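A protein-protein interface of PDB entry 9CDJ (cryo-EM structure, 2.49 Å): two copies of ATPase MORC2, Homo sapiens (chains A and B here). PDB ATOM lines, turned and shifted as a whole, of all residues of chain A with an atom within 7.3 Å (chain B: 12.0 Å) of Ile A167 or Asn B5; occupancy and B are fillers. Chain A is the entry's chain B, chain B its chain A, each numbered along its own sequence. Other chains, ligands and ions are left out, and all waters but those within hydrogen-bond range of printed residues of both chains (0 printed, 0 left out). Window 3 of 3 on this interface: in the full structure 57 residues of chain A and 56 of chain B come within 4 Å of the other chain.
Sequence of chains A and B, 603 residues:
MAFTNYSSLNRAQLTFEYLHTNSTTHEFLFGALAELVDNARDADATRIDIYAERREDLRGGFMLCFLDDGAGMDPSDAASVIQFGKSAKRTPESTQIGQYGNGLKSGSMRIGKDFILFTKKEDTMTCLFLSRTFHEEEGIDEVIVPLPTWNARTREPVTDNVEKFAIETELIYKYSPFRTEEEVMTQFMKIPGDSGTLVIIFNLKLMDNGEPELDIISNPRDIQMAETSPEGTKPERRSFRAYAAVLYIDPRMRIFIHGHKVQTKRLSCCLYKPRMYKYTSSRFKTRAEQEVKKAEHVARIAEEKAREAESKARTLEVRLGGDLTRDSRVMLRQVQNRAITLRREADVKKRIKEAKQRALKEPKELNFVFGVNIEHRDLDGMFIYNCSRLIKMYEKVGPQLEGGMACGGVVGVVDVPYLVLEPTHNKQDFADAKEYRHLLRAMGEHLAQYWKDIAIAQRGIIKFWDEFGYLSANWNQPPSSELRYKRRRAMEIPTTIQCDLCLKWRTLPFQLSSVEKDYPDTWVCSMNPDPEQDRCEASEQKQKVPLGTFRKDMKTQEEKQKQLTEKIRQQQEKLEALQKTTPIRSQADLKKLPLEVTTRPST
The side-chain amide oxygen (OD1) of Asn B10 is in hydrogen-bond range of the side-chain amino group (NZ) of Lys A164, 3.0 Å away.
OH of Tyr B6 sits at hydrogen-bond distance from OE1 of Glu A138.
The backbone NH (N) of Lys A164 is in hydrogen-bond range of the side-chain amide oxygen (OD1) of Asn A161 (2.6 Å).
The backbone carbonyl oxygen (O) of Ser B7 is in hydrogen-bond range of the guanidinium group (NH1) of Arg B11 (3.2 Å).
O of Leu B9 lies within hydrogen-bond range of NH1 of Arg B11, at 3.1 Å.
OD1 of Asn A161 is in hydrogen-bond range of N of Glu A163, 2.9 Å away.
OD1 of Asn B5 sits at hydrogen-bond distance from OG of Ser B7, 2.9 Å away.
The backbone carbonyl oxygen of Tyr B6 sits close to the guanidinium group of Arg B11 (3.3 Å).
Among the printed residues, merely in contact across the chains: Phe A134 with Tyr B6, Ile A144 with Tyr B6, Ile A144 with Leu B9, Ile A144 with Asn B10, Ile A144 with Arg B11, Pro A146 with Leu B9, Asn A161 with Ser B8, Lys A164 with Ser B8, Ile A167 with Asn B5, Ile A167 with Tyr B6, Ile A167 with Leu B9, Glu A168 with Leu B9, Glu A168 with Asn B10, Leu A171 with Tyr B6 and Leu A171 with Leu B9.
Of the printed residues of chain B, Phe A134 touches Tyr B6.
Printed residues of chain B within 4 Å of Glu A138: Tyr B6 (2.5 Å).
Printed residues of chain B within 4 Å of Asn A161: Ser B8 (3.7 Å).
Phe A165 touches none of the printed residues of chain B.
No residue of chain B comes within 4 Å of Ala A166.
Ile A167 touches just these residues of chain B: Asn B5, Tyr B6 and Leu B9.
Glu A168 touches just these residues of chain B: Leu B9 and Asn B10.
Glu A170 touches none of the printed residues of chain B.
Leu A171 touches just these residues of chain B: Tyr B6 (3.4 Å) and Leu B9 (3.4 Å).
Tyr A173 touches none of the printed residues of chain B.
The nearest residue of chain A that does not touch Asn B5 is Glu A138 (6.4 Å).
Of the 17 printed residues of chain A, 9 touch a printed residue of chain B.
Printed residues of chain A that touch a printed residue of chain B: Phe A134, Glu A138, Ile A144, Pro A146, Asn A161, Lys A164, Ile A167, Glu A168 and Leu A171.
Along chain A the printed residues that touch a printed residue of chain B span positions 134 to 171.
Of the 7 printed residues of chain B, 6 touch a printed residue of chain A.
Hydrophobic or aromatic side chains of chain B within 4 Å of the printed part of chain A: Tyr B6 and Leu B9.
Among the printed residues, 17 pairs touch across the chains.
No position is printed for both chains.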
ATOM      1  N   PHE A 134      24.534 -24.993 -20.844  1.00  0.00           N
ATOM      2  CA  PHE A 134      24.597 -23.545 -20.997  1.00  0.00           C
ATOM      3  C   PHE A 134      24.016 -22.845 -19.777  1.00  0.00           C
ATOM      4  O   PHE A 134      24.616 -21.902 -19.245  1.00  0.00           O
ATOM      5  CB  PHE A 134      23.855 -23.139 -22.272  1.00  0.00           C
ATOM      6  CG  PHE A 134      23.416 -21.703 -22.301  1.00  0.00           C
ATOM      7  CD1 PHE A 134      24.311 -20.679 -22.055  1.00  0.00           C
ATOM      8  CD2 PHE A 134      22.101 -21.379 -22.587  1.00  0.00           C
ATOM      9  CE1 PHE A 134      23.900 -19.360 -22.086  1.00  0.00           C
ATOM     10  CE2 PHE A 134      21.687 -20.064 -22.621  1.00  0.00           C
ATOM     11  CZ  PHE A 134      22.588 -19.055 -22.370  1.00  0.00           C
ATOM     12  N   GLU A 138      26.207 -20.522 -17.211  1.00  0.00           N
ATOM     13  CA  GLU A 138      25.956 -19.088 -17.249  1.00  0.00           C
ATOM     14  C   GLU A 138      24.950 -18.630 -16.200  1.00  0.00           C
ATOM     15  O   GLU A 138      24.509 -17.477 -16.243  1.00  0.00           O
ATOM     16  CB  GLU A 138      25.481 -18.685 -18.644  1.00  0.00           C
ATOM     17  CG  GLU A 138      26.487 -19.030 -19.735  1.00  0.00           C
ATOM     18  CD  GLU A 138      26.674 -17.923 -20.755  1.00  0.00           C
ATOM     19  OE1 GLU A 138      26.006 -16.875 -20.643  1.00  0.00           O
ATOM     20  OE2 GLU A 138      27.496 -18.104 -21.677  1.00  0.00           O
ATOM     21  N   ILE A 144      16.374 -20.677 -21.702  1.00  0.00           N
ATOM     22  CA  ILE A 144      16.647 -20.008 -22.967  1.00  0.00           C
ATOM     23  C   ILE A 144      17.059 -21.052 -23.994  1.00  0.00           C
ATOM     24  O   ILE A 144      17.963 -21.860 -23.751  1.00  0.00           O
ATOM     25  CB  ILE A 144      17.738 -18.938 -22.789  1.00  0.00           C
ATOM     26  CG1 ILE A 144      17.266 -17.870 -21.799  1.00  0.00           C
ATOM     27  CG2 ILE A 144      18.086 -18.318 -24.131  1.00  0.00           C
ATOM     28  CD1 ILE A 144      18.339 -16.894 -21.395  1.00  0.00           C
ATOM     29  N   PRO A 146      18.150 -21.336 -27.965  1.00  0.00           N
ATOM     30  CA  PRO A 146      18.425 -20.821 -29.311  1.00  0.00           C
ATOM     31  C   PRO A 146      17.648 -21.591 -30.369  1.00  0.00           C
ATOM     32  O   PRO A 146      17.565 -22.820 -30.331  1.00  0.00           O
ATOM     33  CB  PRO A 146      19.936 -21.023 -29.459  1.00  0.00           C
ATOM     34  CG  PRO A 146      20.455 -20.976 -28.077  1.00  0.00           C
ATOM     35  CD  PRO A 146      19.389 -21.572 -27.205  1.00  0.00           C
ATOM     36  N   ASN A 161      16.276 -10.705 -36.483  1.00  0.00           N
ATOM     37  CA  ASN A 161      17.214 -10.059 -35.568  1.00  0.00           C
ATOM     38  C   ASN A 161      18.581 -10.703 -35.777  1.00  0.00           C
ATOM     39  O   ASN A 161      18.830 -11.826 -35.322  1.00  0.00           O
ATOM     40  CB  ASN A 161      16.734 -10.186 -34.124  1.00  0.00           C
ATOM     41  CG  ASN A 161      17.654  -9.499 -33.134  1.00  0.00           C
ATOM     42  OD1 ASN A 161      18.867  -9.441 -33.326  1.00  0.00           O
ATOM     43  ND2 ASN A 161      17.075  -8.974 -32.060  1.00  0.00           N
ATOM     44  N   VAL A 162      19.470  -9.983 -36.465  1.00  0.00           N
ATOM     45  CA  VAL A 162      20.794 -10.520 -36.762  1.00  0.00           C
ATOM     46  C   VAL A 162      21.572 -10.754 -35.475  1.00  0.00           C
ATOM     47  O   VAL A 162      22.301 -11.744 -35.347  1.00  0.00           O
ATOM     48  CB  VAL A 162      21.557  -9.586 -37.720  1.00  0.00           C
ATOM     49  CG1 VAL A 162      22.761 -10.306 -38.306  1.00  0.00           C
ATOM     50  CG2 VAL A 162      20.648  -9.094 -38.842  1.00  0.00           C
ATOM     51  N   GLU A 163      21.442  -9.846 -34.506  1.00  0.00           N
ATOM     52  CA  GLU A 163      22.121 -10.040 -33.228  1.00  0.00           C
ATOM     53  C   GLU A 163      21.583 -11.271 -32.508  1.00  0.00           C
ATOM     54  O   GLU A 163      22.348 -12.033 -31.904  1.00  0.00           O
ATOM     55  CB  GLU A 163      21.979  -8.799 -32.344  1.00  0.00           C
ATOM     56  CG  GLU A 163      22.048  -7.462 -33.075  1.00  0.00           C
ATOM     57  CD  GLU A 163      20.694  -6.983 -33.567  1.00  0.00           C
ATOM     58  OE1 GLU A 163      19.922  -6.438 -32.751  1.00  0.00           O
ATOM     59  OE2 GLU A 163      20.405  -7.151 -34.771  1.00  0.00           O
ATOM     60  N   LYS A 164      20.267 -11.481 -32.561  1.00  0.00           N
ATOM     61  CA  LYS A 164      19.684 -12.677 -31.962  1.00  0.00           C
ATOM     62  C   LYS A 164      20.251 -13.933 -32.608  1.00  0.00           C
ATOM     63  O   LYS A 164      20.628 -14.886 -31.917  1.00  0.00           O
ATOM     64  CB  LYS A 164      18.163 -12.647 -32.106  1.00  0.00           C
ATOM     65  CG  LYS A 164      17.448 -13.851 -31.506  1.00  0.00           C
ATOM     66  CD  LYS A 164      16.000 -13.907 -31.959  1.00  0.00           C
ATOM     67  CE  LYS A 164      15.228 -14.992 -31.229  1.00  0.00           C
ATOM     68  NZ  LYS A 164      13.756 -14.843 -31.403  1.00  0.00           N
ATOM     69  N   PHE A 165      20.310 -13.953 -33.941  1.00  0.00           N
ATOM     70  CA  PHE A 165      20.851 -15.123 -34.623  1.00  0.00           C
ATOM     71  C   PHE A 165      22.316 -15.336 -34.269  1.00  0.00           C
ATOM     72  O   PHE A 165      22.758 -16.476 -34.087  1.00  0.00           O
ATOM     73  CB  PHE A 165      20.686 -14.983 -36.133  1.00  0.00           C
ATOM     74  CG  PHE A 165      21.260 -16.132 -36.904  1.00  0.00           C
ATOM     75  CD1 PHE A 165      20.508 -17.269 -37.142  1.00  0.00           C
ATOM     76  CD2 PHE A 165      22.559 -16.082 -37.379  1.00  0.00           C
ATOM     77  CE1 PHE A 165      21.038 -18.328 -37.842  1.00  0.00           C
ATOM     78  CE2 PHE A 165      23.092 -17.140 -38.080  1.00  0.00           C
ATOM     79  CZ  PHE A 165      22.331 -18.263 -38.311  1.00  0.00           C
ATOM     80  N   ALA A 166      23.087 -14.254 -34.185  1.00  0.00           N
ATOM     81  CA  ALA A 166      24.494 -14.378 -33.826  1.00  0.00           C
ATOM     82  C   ALA A 166      24.646 -14.979 -32.437  1.00  0.00           C
ATOM     83  O   ALA A 166      25.460 -15.883 -32.226  1.00  0.00           O
ATOM     84  CB  ALA A 166      25.178 -13.013 -33.902  1.00  0.00           C
ATOM     85  N   ILE A 167      23.858 -14.496 -31.477  1.00  0.00           N
ATOM     86  CA  ILE A 167      23.938 -15.030 -30.121  1.00  0.00           C
ATOM     87  C   ILE A 167      23.543 -16.501 -30.107  1.00  0.00           C
ATOM     88  O   ILE A 167      24.185 -17.328 -29.448  1.00  0.00           O
ATOM     89  CB  ILE A 167      23.061 -14.201 -29.166  1.00  0.00           C
ATOM     90  CG1 ILE A 167      23.579 -12.765 -29.076  1.00  0.00           C
ATOM     91  CG2 ILE A 167      23.042 -14.831 -27.783  1.00  0.00           C
ATOM     92  CD1 ILE A 167      22.538 -11.771 -28.618  1.00  0.00           C
ATOM     93  N   GLU A 168      22.477 -16.847 -30.830  1.00  0.00           N
ATOM     94  CA  GLU A 168      22.020 -18.231 -30.875  1.00  0.00           C
ATOM     95  C   GLU A 168      23.099 -19.150 -31.431  1.00  0.00           C
ATOM     96  O   GLU A 168      23.412 -20.194 -30.848  1.00  0.00           O
ATOM     97  CB  GLU A 168      20.753 -18.323 -31.724  1.00  0.00           C
ATOM     98  CG  GLU A 168      19.523 -17.723 -31.073  1.00  0.00           C
ATOM     99  CD  GLU A 168      18.315 -17.744 -31.984  1.00  0.00           C
ATOM    100  OE1 GLU A 168      18.495 -17.627 -33.214  1.00  0.00           O
ATOM    101  OE2 GLU A 168      17.183 -17.878 -31.474  1.00  0.00           O
ATOM    102  N   THR A 169      23.678 -18.772 -32.572  1.00  0.00           N
ATOM    103  CA  THR A 169      24.701 -19.605 -33.192  1.00  0.00           C
ATOM    104  C   THR A 169      25.951 -19.682 -32.325  1.00  0.00           C
ATOM    105  O   THR A 169      26.593 -20.735 -32.252  1.00  0.00           O
ATOM    106  CB  THR A 169      25.044 -19.071 -34.581  1.00  0.00           C
ATOM    107  OG1 THR A 169      25.379 -17.681 -34.495  1.00  0.00           O
ATOM    108  CG2 THR A 169      23.868 -19.256 -35.524  1.00  0.00           C
ATOM    109  N   GLU A 170      26.320 -18.580 -31.671  1.00  0.00           N
ATOM    110  CA  GLU A 170      27.470 -18.615 -30.776  1.00  0.00           C
ATOM    111  C   GLU A 170      27.233 -19.574 -29.620  1.00  0.00           C
ATOM    112  O   GLU A 170      28.121 -20.354 -29.263  1.00  0.00           O
ATOM    113  CB  GLU A 170      27.775 -17.210 -30.259  1.00  0.00           C
ATOM    114  CG  GLU A 170      28.930 -16.521 -30.973  1.00  0.00           C
ATOM    115  CD  GLU A 170      28.765 -16.489 -32.481  1.00  0.00           C
ATOM    116  OE1 GLU A 170      29.751 -16.172 -33.179  1.00  0.00           O
ATOM    117  OE2 GLU A 170      27.658 -16.789 -32.971  1.00  0.00           O
ATOM    118  N   LEU A 171      26.038 -19.542 -29.026  1.00  0.00           N
ATOM    119  CA  LEU A 171      25.733 -20.486 -27.956  1.00  0.00           C
ATOM    120  C   LEU A 171      25.775 -21.919 -28.464  1.00  0.00           C
ATOM    121  O   LEU A 171      26.279 -22.816 -27.775  1.00  0.00           O
ATOM    122  CB  LEU A 171      24.365 -20.183 -27.348  1.00  0.00           C
ATOM    123  CG  LEU A 171      24.230 -18.883 -26.560  1.00  0.00           C
ATOM    124  CD1 LEU A 171      22.805 -18.725 -26.070  1.00  0.00           C
ATOM    125  CD2 LEU A 171      25.204 -18.861 -25.397  1.00  0.00           C
ATOM    126  N   ILE A 172      25.239 -22.161 -29.660  1.00  0.00           N
ATOM    127  CA  ILE A 172      25.257 -23.513 -30.211  1.00  0.00           C
ATOM    128  C   ILE A 172      26.691 -23.991 -30.385  1.00  0.00           C
ATOM    129  O   ILE A 172      27.059 -25.083 -29.939  1.00  0.00           O
ATOM    130  CB  ILE A 172      24.476 -23.563 -31.536  1.00  0.00           C
ATOM    131  CG1 ILE A 172      22.977 -23.460 -31.258  1.00  0.00           C
ATOM    132  CG2 ILE A 172      24.792 -24.846 -32.293  1.00  0.00           C
ATOM    133  CD1 ILE A 172      22.136 -23.299 -32.494  1.00  0.00           C
ATOM    134  N   TYR A 173      27.532 -23.166 -31.007  1.00  0.00           N
ATOM    135  CA  TYR A 173      28.920 -23.559 -31.226  1.00  0.00           C
ATOM    136  C   TYR A 173      29.671 -23.726 -29.912  1.00  0.00           C
ATOM    137  O   TYR A 173      30.573 -24.564 -29.814  1.00  0.00           O
ATOM    138  CB  TYR A 173      29.629 -22.528 -32.106  1.00  0.00           C
ATOM    139  CG  TYR A 173      28.903 -22.194 -33.392  1.00  0.00           C
ATOM    140  CD1 TYR A 173      28.059 -23.114 -33.999  1.00  0.00           C
ATOM    141  CD2 TYR A 173      29.062 -20.956 -33.998  1.00  0.00           C
ATOM    142  CE1 TYR A 173      27.396 -22.810 -35.171  1.00  0.00           C
ATOM    143  CE2 TYR A 173      28.404 -20.644 -35.169  1.00  0.00           C
ATOM    144  CZ  TYR A 173      27.572 -21.574 -35.751  1.00  0.00           C
ATOM    145  OH  TYR A 173      26.914 -21.267 -36.918  1.00  0.00           O
ATOM    146  N   ASN B   5      24.296 -11.128 -22.990  1.00  0.00           N
ATOM    147  CA  ASN B   5      22.877 -10.824 -22.851  1.00  0.00           C
ATOM    148  C   ASN B   5      22.052 -11.693 -23.792  1.00  0.00           C
ATOM    149  O   ASN B   5      22.381 -11.832 -24.969  1.00  0.00           O
ATOM    150  CB  ASN B   5      22.617  -9.344 -23.135  1.00  0.00           C
ATOM    151  CG  ASN B   5      21.160  -8.966 -22.959  1.00  0.00           C
ATOM    152  OD1 ASN B   5      20.440  -8.749 -23.934  1.00  0.00           O
ATOM    153  ND2 ASN B   5      20.718  -8.884 -21.710  1.00  0.00           N
ATOM    154  N   TYR B   6      20.974 -12.275 -23.264  1.00  0.00           N
ATOM    155  CA  TYR B   6      20.123 -13.186 -24.021  1.00  0.00           C
ATOM    156  C   TYR B   6      18.669 -12.733 -23.998  1.00  0.00           C
ATOM    157  O   TYR B   6      17.756 -13.553 -24.123  1.00  0.00           O
ATOM    158  CB  TYR B   6      20.242 -14.610 -23.483  1.00  0.00           C
ATOM    159  CG  TYR B   6      21.667 -15.089 -23.361  1.00  0.00           C
ATOM    160  CD1 TYR B   6      22.454 -15.272 -24.487  1.00  0.00           C
ATOM    161  CD2 TYR B   6      22.228 -15.352 -22.121  1.00  0.00           C
ATOM    162  CE1 TYR B   6      23.758 -15.704 -24.382  1.00  0.00           C
ATOM    163  CE2 TYR B   6      23.531 -15.787 -22.006  1.00  0.00           C
ATOM    164  CZ  TYR B   6      24.292 -15.960 -23.141  1.00  0.00           C
ATOM    165  OH  TYR B   6      25.593 -16.393 -23.038  1.00  0.00           O
ATOM    166  N   SER B   7      18.436 -11.429 -23.841  1.00  0.00           N
ATOM    167  CA  SER B   7      17.066 -10.930 -23.808  1.00  0.00           C
ATOM    168  C   SER B   7      16.336 -11.217 -25.112  1.00  0.00           C
ATOM    169  O   SER B   7      15.118 -11.430 -25.108  1.00  0.00           O
ATOM    170  CB  SER B   7      17.066  -9.429 -23.520  1.00  0.00           C
ATOM    171  OG  SER B   7      17.637  -8.705 -24.595  1.00  0.00           O
ATOM    172  N   SER B   8      17.056 -11.226 -26.234  1.00  0.00           N
ATOM    173  CA  SER B   8      16.437 -11.460 -27.531  1.00  0.00           C
ATOM    174  C   SER B   8      16.076 -12.920 -27.764  1.00  0.00           C
ATOM    175  O   SER B   8      15.187 -13.201 -28.574  1.00  0.00           O
ATOM    176  CB  SER B   8      17.370 -10.990 -28.647  1.00  0.00           C
ATOM    177  OG  SER B   8      17.677  -9.615 -28.513  1.00  0.00           O
ATOM    178  N   LEU B   9      16.734 -13.848 -27.076  1.00  0.00           N
ATOM    179  CA  LEU B   9      16.584 -15.262 -27.379  1.00  0.00           C
ATOM    180  C   LEU B   9      15.222 -15.782 -26.941  1.00  0.00           C
ATOM    181  O   LEU B   9      14.578 -15.236 -26.040  1.00  0.00           O
ATOM    182  CB  LEU B   9      17.682 -16.076 -26.699  1.00  0.00           C
ATOM    183  CG  LEU B   9      18.904 -16.366 -27.568  1.00  0.00           C
ATOM    184  CD1 LEU B   9      19.686 -15.091 -27.828  1.00  0.00           C
ATOM    185  CD2 LEU B   9      19.785 -17.414 -26.916  1.00  0.00           C
ATOM    186  N   ASN B  10      14.788 -16.858 -27.594  1.00  0.00           N
ATOM    187  CA  ASN B  10      13.529 -17.496 -27.241  1.00  0.00           C
ATOM    188  C   ASN B  10      13.614 -18.102 -25.846  1.00  0.00           C
ATOM    189  O   ASN B  10      14.684 -18.495 -25.375  1.00  0.00           O
ATOM    190  CB  ASN B  10      13.180 -18.585 -28.257  1.00  0.00           C
ATOM    191  CG  ASN B  10      12.770 -18.019 -29.598  1.00  0.00           C
ATOM    192  OD1 ASN B  10      13.615 -17.665 -30.419  1.00  0.00           O
ATOM    193  ND2 ASN B  10      11.466 -17.939 -29.832  1.00  0.00           N
ATOM    194  N   ARG B  11      12.465 -18.172 -25.183  1.00  0.00           N
ATOM    195  CA  ARG B  11      12.352 -18.744 -23.850  1.00  0.00           C
ATOM    196  C   ARG B  11      11.365 -19.899 -23.887  1.00  0.00           C
ATOM    197  O   ARG B  11      10.311 -19.801 -24.522  1.00  0.00           O
ATOM    198  CB  ARG B  11      11.878 -17.696 -22.838  1.00  0.00           C
ATOM    199  CG  ARG B  11      12.970 -17.153 -21.937  1.00  0.00           C
ATOM    200  CD  ARG B  11      13.665 -15.974 -22.590  1.00  0.00           C
ATOM    201  NE  ARG B  11      14.602 -15.315 -21.690  1.00  0.00           N
ATOM    202  CZ  ARG B  11      15.500 -14.418 -22.073  1.00  0.00           C
ATOM    203  NH1 ARG B  11      15.610 -14.047 -23.338  1.00  0.00           N
ATOM    204  NH2 ARG B  11      16.307 -13.879 -21.164  1.00  0.00           N
